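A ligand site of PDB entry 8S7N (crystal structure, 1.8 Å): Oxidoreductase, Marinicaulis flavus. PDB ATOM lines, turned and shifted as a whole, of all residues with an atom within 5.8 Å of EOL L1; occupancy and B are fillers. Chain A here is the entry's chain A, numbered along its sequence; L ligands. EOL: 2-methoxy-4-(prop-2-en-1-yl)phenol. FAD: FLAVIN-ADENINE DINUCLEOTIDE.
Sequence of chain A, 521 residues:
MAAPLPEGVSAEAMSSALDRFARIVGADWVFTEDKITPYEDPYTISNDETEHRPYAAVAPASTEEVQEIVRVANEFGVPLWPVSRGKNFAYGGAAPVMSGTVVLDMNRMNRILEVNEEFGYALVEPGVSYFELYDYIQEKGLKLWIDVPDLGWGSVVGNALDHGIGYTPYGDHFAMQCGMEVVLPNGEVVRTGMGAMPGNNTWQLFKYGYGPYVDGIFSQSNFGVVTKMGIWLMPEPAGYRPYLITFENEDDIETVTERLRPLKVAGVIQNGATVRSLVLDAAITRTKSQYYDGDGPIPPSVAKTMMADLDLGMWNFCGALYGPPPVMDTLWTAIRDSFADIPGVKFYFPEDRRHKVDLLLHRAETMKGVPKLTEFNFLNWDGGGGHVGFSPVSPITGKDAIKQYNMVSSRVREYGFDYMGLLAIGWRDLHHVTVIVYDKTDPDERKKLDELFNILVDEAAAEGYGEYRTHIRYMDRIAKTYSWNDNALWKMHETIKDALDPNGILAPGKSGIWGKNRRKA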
ATOM      1  N   PHE A  89      -1.997 -11.087 -24.664  1.00  0.00           N
ATOM      2  CA  PHE A  89      -1.584  -9.957 -25.544  1.00  0.00           C
ATOM      3  C   PHE A  89      -2.833  -9.411 -26.255  1.00  0.00           C
ATOM      4  O   PHE A  89      -3.674 -10.238 -26.664  1.00  0.00           O
ATOM      5  CB  PHE A  89      -0.505 -10.442 -26.502  1.00  0.00           C
ATOM      6  CG  PHE A  89       0.696 -11.005 -25.792  1.00  0.00           C
ATOM      7  CD1 PHE A  89       1.154 -10.437 -24.620  1.00  0.00           C
ATOM      8  CD2 PHE A  89       1.259 -12.182 -26.215  1.00  0.00           C
ATOM      9  CE1 PHE A  89       2.219 -10.987 -23.915  1.00  0.00           C
ATOM     10  CE2 PHE A  89       2.306 -12.743 -25.509  1.00  0.00           C
ATOM     11  CZ  PHE A  89       2.802 -12.124 -24.391  1.00  0.00           C
ATOM     12  N   ALA A  90      -2.913  -8.083 -26.319  1.00  0.00           N
ATOM     13  CA  ALA A  90      -4.065  -7.256 -26.811  1.00  0.00           C
ATOM     14  C   ALA A  90      -5.048  -7.012 -25.650  1.00  0.00           C
ATOM     15  O   ALA A  90      -5.906  -6.085 -25.810  1.00  0.00           O
ATOM     16  CB  ALA A  90      -4.727  -7.875 -28.009  1.00  0.00           C
ATOM     17  N   TYR A  91      -4.832  -7.652 -24.484  1.00  0.00           N
ATOM     18  CA  TYR A  91      -5.627  -7.367 -23.265  1.00  0.00           C
ATOM     19  C   TYR A  91      -4.739  -7.044 -22.060  1.00  0.00           C
ATOM     20  O   TYR A  91      -5.283  -7.006 -20.932  1.00  0.00           O
ATOM     21  CB  TYR A  91      -6.552  -8.545 -23.005  1.00  0.00           C
ATOM     22  CG  TYR A  91      -7.632  -8.771 -24.059  1.00  0.00           C
ATOM     23  CD1 TYR A  91      -8.465  -7.731 -24.487  1.00  0.00           C
ATOM     24  CD2 TYR A  91      -7.869 -10.043 -24.565  1.00  0.00           C
ATOM     25  CE1 TYR A  91      -9.475  -7.965 -25.399  1.00  0.00           C
ATOM     26  CE2 TYR A  91      -8.851 -10.269 -25.529  1.00  0.00           C
ATOM     27  CZ  TYR A  91      -9.696  -9.244 -25.889  1.00  0.00           C
ATOM     28  OH  TYR A  91     -10.674  -9.512 -26.807  1.00  0.00           O
ATOM     29  N   ASP A 150      -6.182 -18.365 -32.126  1.00  0.00           N
ATOM     30  CA  ASP A 150      -5.220 -18.105 -33.225  1.00  0.00           C
ATOM     31  C   ASP A 150      -3.783 -18.356 -32.711  1.00  0.00           C
ATOM     32  O   ASP A 150      -2.940 -18.690 -33.533  1.00  0.00           O
ATOM     33  CB  ASP A 150      -5.349 -16.691 -33.774  1.00  0.00           C
ATOM     34  CG  ASP A 150      -6.598 -16.482 -34.595  1.00  0.00           C
ATOM     35  OD1 ASP A 150      -6.985 -17.410 -35.368  1.00  0.00           O
ATOM     36  OD2 ASP A 150      -7.138 -15.385 -34.473  1.00  0.00           O
ATOM     37  N   ILE A 165     -11.998 -17.983 -27.188  1.00  0.00           N
ATOM     38  CA  ILE A 165     -12.691 -18.680 -28.290  1.00  0.00           C
ATOM     39  C   ILE A 165     -11.694 -19.263 -29.270  1.00  0.00           C
ATOM     40  O   ILE A 165     -10.624 -18.710 -29.500  1.00  0.00           O
ATOM     41  CB  ILE A 165     -13.691 -17.732 -28.979  1.00  0.00           C
ATOM     42  CG1 ILE A 165     -13.014 -16.518 -29.611  1.00  0.00           C
ATOM     43  CG2 ILE A 165     -14.744 -17.306 -27.966  1.00  0.00           C
ATOM     44  CD1 ILE A 165     -13.983 -15.650 -30.418  1.00  0.00           C
ATOM     45  N   TYR A 167     -12.114 -22.273 -32.997  1.00  0.00           N
ATOM     46  CA  TYR A 167     -12.598 -22.293 -34.400  1.00  0.00           C
ATOM     47  C   TYR A 167     -13.038 -23.669 -34.828  1.00  0.00           C
ATOM     48  O   TYR A 167     -13.225 -23.838 -36.049  1.00  0.00           O
ATOM     49  CB  TYR A 167     -11.583 -21.601 -35.304  1.00  0.00           C
ATOM     50  CG  TYR A 167     -11.250 -20.216 -34.789  1.00  0.00           C
ATOM     51  CD1 TYR A 167     -12.191 -19.205 -34.872  1.00  0.00           C
ATOM     52  CD2 TYR A 167     -10.034 -19.938 -34.157  1.00  0.00           C
ATOM     53  CE1 TYR A 167     -11.941 -17.951 -34.336  1.00  0.00           C
ATOM     54  CE2 TYR A 167      -9.751 -18.683 -33.638  1.00  0.00           C
ATOM     55  CZ  TYR A 167     -10.714 -17.692 -33.707  1.00  0.00           C
ATOM     56  OH  TYR A 167     -10.479 -16.473 -33.173  1.00  0.00           O
ATOM     57  N   ARG A 276     -14.531 -12.378 -41.610  1.00  0.00           N
ATOM     58  CA  ARG A 276     -13.347 -11.511 -41.341  1.00  0.00           C
ATOM     59  C   ARG A 276     -13.291 -10.468 -42.461  1.00  0.00           C
ATOM     60  O   ARG A 276     -13.631 -10.782 -43.593  1.00  0.00           O
ATOM     61  CB  ARG A 276     -12.091 -12.403 -41.206  1.00  0.00           C
ATOM     62  CG  ARG A 276     -11.996 -13.097 -39.848  1.00  0.00           C
ATOM     63  CD  ARG A 276     -10.992 -14.267 -39.702  1.00  0.00           C
ATOM     64  NE  ARG A 276      -9.690 -13.886 -40.201  1.00  0.00           N
ATOM     65  CZ  ARG A 276      -8.553 -13.741 -39.473  1.00  0.00           C
ATOM     66  NH1 ARG A 276      -8.536 -13.904 -38.167  1.00  0.00           N
ATOM     67  NH2 ARG A 276      -7.416 -13.406 -40.100  1.00  0.00           N
ATOM     68  N   LEU A 280      -8.057  -7.514 -42.383  1.00  0.00           N
ATOM     69  CA  LEU A 280      -7.611  -8.528 -41.396  1.00  0.00           C
ATOM     70  C   LEU A 280      -7.084  -9.732 -42.178  1.00  0.00           C
ATOM     71  O   LEU A 280      -6.033 -10.304 -41.820  1.00  0.00           O
ATOM     72  CB  LEU A 280      -8.788  -8.892 -40.489  1.00  0.00           C
ATOM     73  CG  LEU A 280      -8.477  -9.990 -39.473  1.00  0.00           C
ATOM     74  CD1 LEU A 280      -7.221  -9.689 -38.673  1.00  0.00           C
ATOM     75  CD2 LEU A 280      -9.689 -10.161 -38.562  1.00  0.00           C
ATOM     76  N   GLU A 375      -0.870 -15.777 -36.788  1.00  0.00           N
ATOM     77  CA  GLU A 375      -1.839 -14.670 -36.726  1.00  0.00           C
ATOM     78  C   GLU A 375      -1.158 -13.334 -36.417  1.00  0.00           C
ATOM     79  O   GLU A 375      -1.714 -12.305 -36.807  1.00  0.00           O
ATOM     80  CB  GLU A 375      -2.962 -15.002 -35.735  1.00  0.00           C
ATOM     81  CG  GLU A 375      -4.195 -14.198 -36.019  1.00  0.00           C
ATOM     82  CD  GLU A 375      -4.926 -14.422 -37.338  1.00  0.00           C
ATOM     83  OE1 GLU A 375      -4.812 -15.525 -37.900  1.00  0.00           O
ATOM     84  OE2 GLU A 375      -5.688 -13.479 -37.744  1.00  0.00           O
ATOM     85  N   PHE A 378      -0.614 -10.084 -38.938  1.00  0.00           N
ATOM     86  CA  PHE A 378      -1.381  -8.856 -39.258  1.00  0.00           C
ATOM     87  C   PHE A 378      -0.724  -7.629 -38.618  1.00  0.00           C
ATOM     88  O   PHE A 378      -1.019  -6.496 -39.055  1.00  0.00           O
ATOM     89  CB  PHE A 378      -2.879  -9.028 -39.010  1.00  0.00           C
ATOM     90  CG  PHE A 378      -3.348  -9.093 -37.590  1.00  0.00           C
ATOM     91  CD1 PHE A 378      -3.169  -8.028 -36.725  1.00  0.00           C
ATOM     92  CD2 PHE A 378      -4.063 -10.200 -37.149  1.00  0.00           C
ATOM     93  CE1 PHE A 378      -3.641  -8.058 -35.424  1.00  0.00           C
ATOM     94  CE2 PHE A 378      -4.544 -10.236 -35.848  1.00  0.00           C
ATOM     95  CZ  PHE A 378      -4.327  -9.174 -34.986  1.00  0.00           C
ATOM     96  N   HIS A 387      -1.458  -4.415 -30.800  1.00  0.00           N
ATOM     97  CA  HIS A 387      -2.906  -4.362 -31.089  1.00  0.00           C
ATOM     98  C   HIS A 387      -3.657  -4.394 -29.767  1.00  0.00           C
ATOM     99  O   HIS A 387      -3.059  -4.726 -28.729  1.00  0.00           O
ATOM    100  CB  HIS A 387      -3.306  -5.440 -32.102  1.00  0.00           C
ATOM    101  CG  HIS A 387      -3.493  -6.817 -31.594  1.00  0.00           C
ATOM    102  ND1 HIS A 387      -4.746  -7.411 -31.570  1.00  0.00           N
ATOM    103  CD2 HIS A 387      -2.612  -7.763 -31.190  1.00  0.00           C
ATOM    104  CE1 HIS A 387      -4.626  -8.667 -31.193  1.00  0.00           C
ATOM    105  NE2 HIS A 387      -3.313  -8.924 -30.921  1.00  0.00           N
ATOM    106  N   VAL A 388      -4.879  -3.941 -29.835  1.00  0.00           N
ATOM    107  CA  VAL A 388      -5.842  -4.064 -28.708  1.00  0.00           C
ATOM    108  C   VAL A 388      -7.160  -4.558 -29.315  1.00  0.00           C
ATOM    109  O   VAL A 388      -7.463  -4.219 -30.469  1.00  0.00           O
ATOM    110  CB  VAL A 388      -5.976  -2.738 -27.948  1.00  0.00           C
ATOM    111  CG1 VAL A 388      -6.613  -1.669 -28.824  1.00  0.00           C
ATOM    112  CG2 VAL A 388      -6.761  -2.928 -26.653  1.00  0.00           C
ATOM    113  N   GLY A 389      -7.887  -5.369 -28.549  1.00  0.00           N
ATOM    114  CA  GLY A 389      -9.154  -5.919 -29.012  1.00  0.00           C
ATOM    115  C   GLY A 389     -10.313  -5.099 -28.468  1.00  0.00           C
ATOM    116  O   GLY A 389     -10.465  -5.009 -27.263  1.00  0.00           O
ATOM    117  N   SER A 391     -14.099  -5.593 -28.312  1.00  0.00           N
ATOM    118  CA  SER A 391     -14.796  -6.872 -28.494  1.00  0.00           C
ATOM    119  C   SER A 391     -16.262  -6.851 -28.049  1.00  0.00           C
ATOM    120  O   SER A 391     -16.636  -7.616 -27.137  1.00  0.00           O
ATOM    121  CB  SER A 391     -14.030  -7.928 -27.688  1.00  0.00           C
ATOM    122  OG  SER A 391     -12.604  -7.804 -27.856  1.00  0.00           O
ATOM    123  N   LEU A 422     -13.346  -9.038 -36.977  1.00  0.00           N
ATOM    124  CA  LEU A 422     -13.713 -10.477 -36.904  1.00  0.00           C
ATOM    125  C   LEU A 422     -15.127 -10.529 -36.298  1.00  0.00           C
ATOM    126  O   LEU A 422     -15.343  -9.937 -35.230  1.00  0.00           O
ATOM    127  CB  LEU A 422     -12.689 -11.177 -35.995  1.00  0.00           C
ATOM    128  CG  LEU A 422     -13.148 -12.501 -35.377  1.00  0.00           C
ATOM    129  CD1 LEU A 422     -13.415 -13.516 -36.465  1.00  0.00           C
ATOM    130  CD2 LEU A 422     -12.158 -13.081 -34.375  1.00  0.00           C
ATOM    131  N   VAL A 433     -14.871  -8.850 -32.769  1.00  0.00           N
ATOM    132  CA  VAL A 433     -13.542  -8.420 -32.267  1.00  0.00           C
ATOM    133  C   VAL A 433     -12.891  -7.545 -33.354  1.00  0.00           C
ATOM    134  O   VAL A 433     -12.632  -8.052 -34.401  1.00  0.00           O
ATOM    135  CB  VAL A 433     -12.672  -9.640 -31.901  1.00  0.00           C
ATOM    136  CG1 VAL A 433     -11.320  -9.204 -31.332  1.00  0.00           C
ATOM    137  CG2 VAL A 433     -13.375 -10.529 -30.859  1.00  0.00           C
ATOM    138  N   VAL A 435      -9.515  -5.739 -34.122  1.00  0.00           N
ATOM    139  CA  VAL A 435      -8.101  -5.628 -33.669  1.00  0.00           C
ATOM    140  C   VAL A 435      -7.550  -4.338 -34.261  1.00  0.00           C
ATOM    141  O   VAL A 435      -7.596  -4.160 -35.491  1.00  0.00           O
ATOM    142  CB  VAL A 435      -7.308  -6.892 -34.015  1.00  0.00           C
ATOM    143  CG1 VAL A 435      -7.786  -8.028 -33.112  1.00  0.00           C
ATOM    144  CG2 VAL A 435      -7.411  -7.275 -35.471  1.00  0.00           C
ATOM    145  N   TYR A 468     -17.389  -8.481 -24.319  1.00  0.00           N
ATOM    146  CA  TYR A 468     -17.288  -9.799 -23.626  1.00  0.00           C
ATOM    147  C   TYR A 468     -15.954  -9.881 -22.865  1.00  0.00           C
ATOM    148  O   TYR A 468     -15.804 -10.759 -21.949  1.00  0.00           O
ATOM    149  CB  TYR A 468     -17.490 -10.972 -24.618  1.00  0.00           C
ATOM    150  CG  TYR A 468     -16.232 -11.535 -25.233  1.00  0.00           C
ATOM    151  CD1 TYR A 468     -15.505 -10.897 -26.250  1.00  0.00           C
ATOM    152  CD2 TYR A 468     -15.715 -12.724 -24.752  1.00  0.00           C
ATOM    153  CE1 TYR A 468     -14.300 -11.402 -26.744  1.00  0.00           C
ATOM    154  CE2 TYR A 468     -14.516 -13.236 -25.223  1.00  0.00           C
ATOM    155  CZ  TYR A 468     -13.817 -12.612 -26.261  1.00  0.00           C
ATOM    156  OH  TYR A 468     -12.613 -13.204 -26.662  1.00  0.00           O
ATOM    157  N   ARG A 469     -14.979  -9.066 -23.252  1.00  0.00           N
ATOM    158  CA  ARG A 469     -13.578  -9.185 -22.788  1.00  0.00           C
ATOM    159  C   ARG A 469     -12.858  -7.880 -23.071  1.00  0.00           C
ATOM    160  O   ARG A 469     -13.174  -7.200 -24.117  1.00  0.00           O
ATOM    161  CB  ARG A 469     -12.956 -10.366 -23.509  1.00  0.00           C
ATOM    162  CG  ARG A 469     -11.627 -10.863 -22.973  1.00  0.00           C
ATOM    163  CD  ARG A 469     -11.253 -12.068 -23.799  1.00  0.00           C
ATOM    164  NE  ARG A 469      -9.942 -12.626 -23.437  1.00  0.00           N
ATOM    165  CZ  ARG A 469      -9.354 -13.593 -24.107  1.00  0.00           C
ATOM    166  NH1 ARG A 469      -9.973 -14.099 -25.166  1.00  0.00           N
ATOM    167  NH2 ARG A 469      -8.166 -14.045 -23.758  1.00  0.00           N
HETATM  168  C1  EOL L   1      -8.630 -11.713 -30.876  1.00  0.00           C
HETATM  169  O1  EOL L   1     -10.822 -11.813 -27.935  1.00  0.00           O
HETATM  170  C2  EOL L   1      -9.197 -12.692 -31.682  1.00  0.00           C
HETATM  171  O2  EOL L   1      -8.740 -10.498 -28.731  1.00  0.00           O
HETATM  172  C3  EOL L   1      -9.152 -11.449 -29.607  1.00  0.00           C
HETATM  173  C4  EOL L   1     -10.268 -13.417 -31.180  1.00  0.00           C
HETATM  174  C5  EOL L   1     -10.256 -12.180 -29.130  1.00  0.00           C
HETATM  175  C6  EOL L   1     -10.810 -13.163 -29.932  1.00  0.00           C
HETATM  176  C7  EOL L   1      -8.609 -13.052 -33.036  1.00  0.00           C
HETATM  177  C8  EOL L   1      -8.300 -11.925 -33.920  1.00  0.00           C
HETATM  178  C9  EOL L   1      -7.612 -12.023 -35.016  1.00  0.00           C
HETATM  179  C10 EOL L   1      -7.848  -9.490 -29.163  1.00  0.00           C
HETATM  180  PA  FAD L   2      -3.538 -15.945 -19.360  1.00  0.00           P
HETATM  181  O1A FAD L   2      -2.820 -14.682 -19.735  1.00  0.00           O
HETATM  182  O2A FAD L   2      -2.748 -16.902 -18.530  1.00  0.00           O
HETATM  183  O5B FAD L   2      -4.917 -15.634 -18.572  1.00  0.00           O
HETATM  184  C5B FAD L   2      -5.780 -14.562 -18.973  1.00  0.00           C
HETATM  185  C4B FAD L   2      -6.320 -13.903 -17.722  1.00  0.00           C
HETATM  186  O4B FAD L   2      -7.243 -14.803 -17.053  1.00  0.00           O
HETATM  187  C3B FAD L   2      -5.304 -13.511 -16.627  1.00  0.00           C
HETATM  188  O3B FAD L   2      -4.835 -12.194 -16.868  1.00  0.00           O
HETATM  189  C2B FAD L   2      -6.180 -13.572 -15.368  1.00  0.00           C
HETATM  190  O2B FAD L   2      -6.974 -12.420 -15.219  1.00  0.00           O
HETATM  191  C1B FAD L   2      -7.045 -14.775 -15.655  1.00  0.00           C
HETATM  192  N9A FAD L   2      -6.440 -16.057 -15.225  1.00  0.00           N
HETATM  193  C8A FAD L   2      -5.724 -16.878 -16.031  1.00  0.00           C
HETATM  194  N7A FAD L   2      -5.344 -17.986 -15.428  1.00  0.00           N
HETATM  195  C5A FAD L   2      -5.902 -17.896 -14.159  1.00  0.00           C
HETATM  196  C6A FAD L   2      -5.904 -18.801 -13.088  1.00  0.00           C
HETATM  197  N6A FAD L   2      -5.307 -19.991 -13.159  1.00  0.00           N
HETATM  198  N1A FAD L   2      -6.588 -18.456 -11.978  1.00  0.00           N
HETATM  199  C2A FAD L   2      -7.190 -17.244 -11.968  1.00  0.00           C
HETATM  200  N3A FAD L   2      -7.275 -16.322 -12.932  1.00  0.00           N
HETATM  201  C4A FAD L   2      -6.606 -16.720 -14.026  1.00  0.00           C
HETATM  202  N1  FAD L   2      -7.959 -14.867 -27.854  1.00  0.00           N
HETATM  203  C2  FAD L   2      -8.876 -15.827 -28.114  1.00  0.00           C
HETATM  204  O2  FAD L   2      -9.633 -16.228 -27.202  1.00  0.00           O
HETATM  205  N3  FAD L   2      -9.034 -16.358 -29.400  1.00  0.00           N
HETATM  206  C4  FAD L   2      -8.211 -15.981 -30.463  1.00  0.00           C
HETATM  207  O4  FAD L   2      -8.369 -16.499 -31.573  1.00  0.00           O
HETATM  208  C4X FAD L   2      -7.264 -14.955 -30.211  1.00  0.00           C
HETATM  209  N5  FAD L   2      -6.434 -14.564 -31.193  1.00  0.00           N
HETATM  210  C5X FAD L   2      -5.560 -13.552 -30.926  1.00  0.00           C
HETATM  211  C6  FAD L   2      -4.758 -13.062 -31.988  1.00  0.00           C
HETATM  212  C7  FAD L   2      -3.862 -12.015 -31.815  1.00  0.00           C
HETATM  213  C7M FAD L   2      -2.983 -11.562 -32.959  1.00  0.00           C
HETATM  214  C8  FAD L   2      -3.750 -11.408 -30.550  1.00  0.00           C
HETATM  215  C8M FAD L   2      -2.868 -10.185 -30.385  1.00  0.00           C
HETATM  216  C9  FAD L   2      -4.527 -11.901 -29.472  1.00  0.00           C
HETATM  217  C9A FAD L   2      -5.434 -12.966 -29.641  1.00  0.00           C
HETATM  218  N10 FAD L   2      -6.224 -13.478 -28.591  1.00  0.00           N
HETATM  219  C10 FAD L   2      -7.183 -14.464 -28.848  1.00  0.00           C
HETATM  220  C1' FAD L   2      -6.133 -12.907 -27.233  1.00  0.00           C
HETATM  221  C2' FAD L   2      -5.087 -13.547 -26.330  1.00  0.00           C
HETATM  222  O2' FAD L   2      -3.784 -13.283 -26.811  1.00  0.00           O
HETATM  223  C3' FAD L   2      -5.254 -15.079 -26.151  1.00  0.00           C
HETATM  224  O3' FAD L   2      -6.609 -15.340 -25.733  1.00  0.00           O
HETATM  225  C4' FAD L   2      -4.287 -15.756 -25.163  1.00  0.00           C
HETATM  226  O4' FAD L   2      -4.407 -17.175 -25.281  1.00  0.00           O
HETATM  227  C5' FAD L   2      -4.583 -15.448 -23.713  1.00  0.00           C
HETATM  228  O5' FAD L   2      -3.384 -15.668 -22.874  1.00  0.00           O
HETATM  229  P   FAD L   2      -3.202 -17.015 -22.073  1.00  0.00           P
HETATM  230  O1P FAD L   2      -3.872 -18.162 -22.742  1.00  0.00           O
HETATM  231  O2P FAD L   2      -1.730 -17.144 -21.733  1.00  0.00           O
HETATM  232  O3P FAD L   2      -4.021 -16.699 -20.719  1.00  0.00           O
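The guanidinium group of Arg 469 is in hydrogen-bond range of an oxygen (O3') of FAD L2 (2.8 Å). A nitrogen (N3) of FAD L2 lies within hydrogen-bond range of the backbone carbonyl oxygen (O) of Ile 165 (2.8 Å). The side-chain hydroxyl (OH) of Tyr 91 is in hydrogen-bond range of an oxygen (O1) of EOL L1 (2.6 Å). An oxygen (O2) of FAD L2 is in hydrogen-bond range of the backbone NH (N) of Ile 165 (2.9 Å). The side-chain hydroxyl (OH) of Tyr 167 sits at hydrogen-bond distance from an oxygen (O4) of FAD L2, 2.6 Å away. O4 of FAD L2 lies within hydrogen-bond range of N of Asp 150 (2.9 Å). The backbone carbonyl oxygen of Phe 89 sits at hydrogen-bond distance from an oxygen (O2') of FAD L2, 3.1 Å away. A ring nitrogen (NE2) of His 387 is bonded to a carbon (C8M) of FAD L2 (1.4 Å). The side-chain hydroxyl (OH) of Tyr 468 sits at hydrogen-bond distance from an oxygen (O1) of EOL L1 (2.6 Å).
O of Ser 391 lies within hydrogen-bond range of N of Tyr 468 (3.0 Å). The side-chain carboxylate of Glu 375 is in salt-bridge range of the guanidinium group of Arg 276 (2.9 Å). N of Val 433 lies within hydrogen-bond range of O of Leu 422, at 2.7 Å. O of Ala 90 sits at hydrogen-bond distance from N of Gly 389, at 3.5 Å. OH of Tyr 468 is in hydrogen-bond range of NH1 of Arg 469 (3.2 Å). OH of Tyr 91 is in hydrogen-bond range of OG of Ser 391 (2.8 Å).
Merely in contact with EOL L1: Ala 90 (3.7 Å), Asp 150 (3.1 Å), Tyr 167 (3.7 Å), Arg 276 (3.8 Å), Glu 375 (3.6 Å), Phe 378 (3.6 Å), His 387 (3.9 Å), Gly 389 (3.8 Å), Leu 422 (3.7 Å), Val 433 (3.6 Å) and Arg 469 (3.7 Å). Hydrophobic or aromatic side chains that line EOL L1: Ala 90, Tyr 91, Phe 378, His 387, Leu 422, Val 433 and Tyr 468. Of the 19 residues printed, 13 come within 4 Å of EOL L1. The nearest printed residue that does not touch EOL L1 is Val 435 (4.01 Å).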
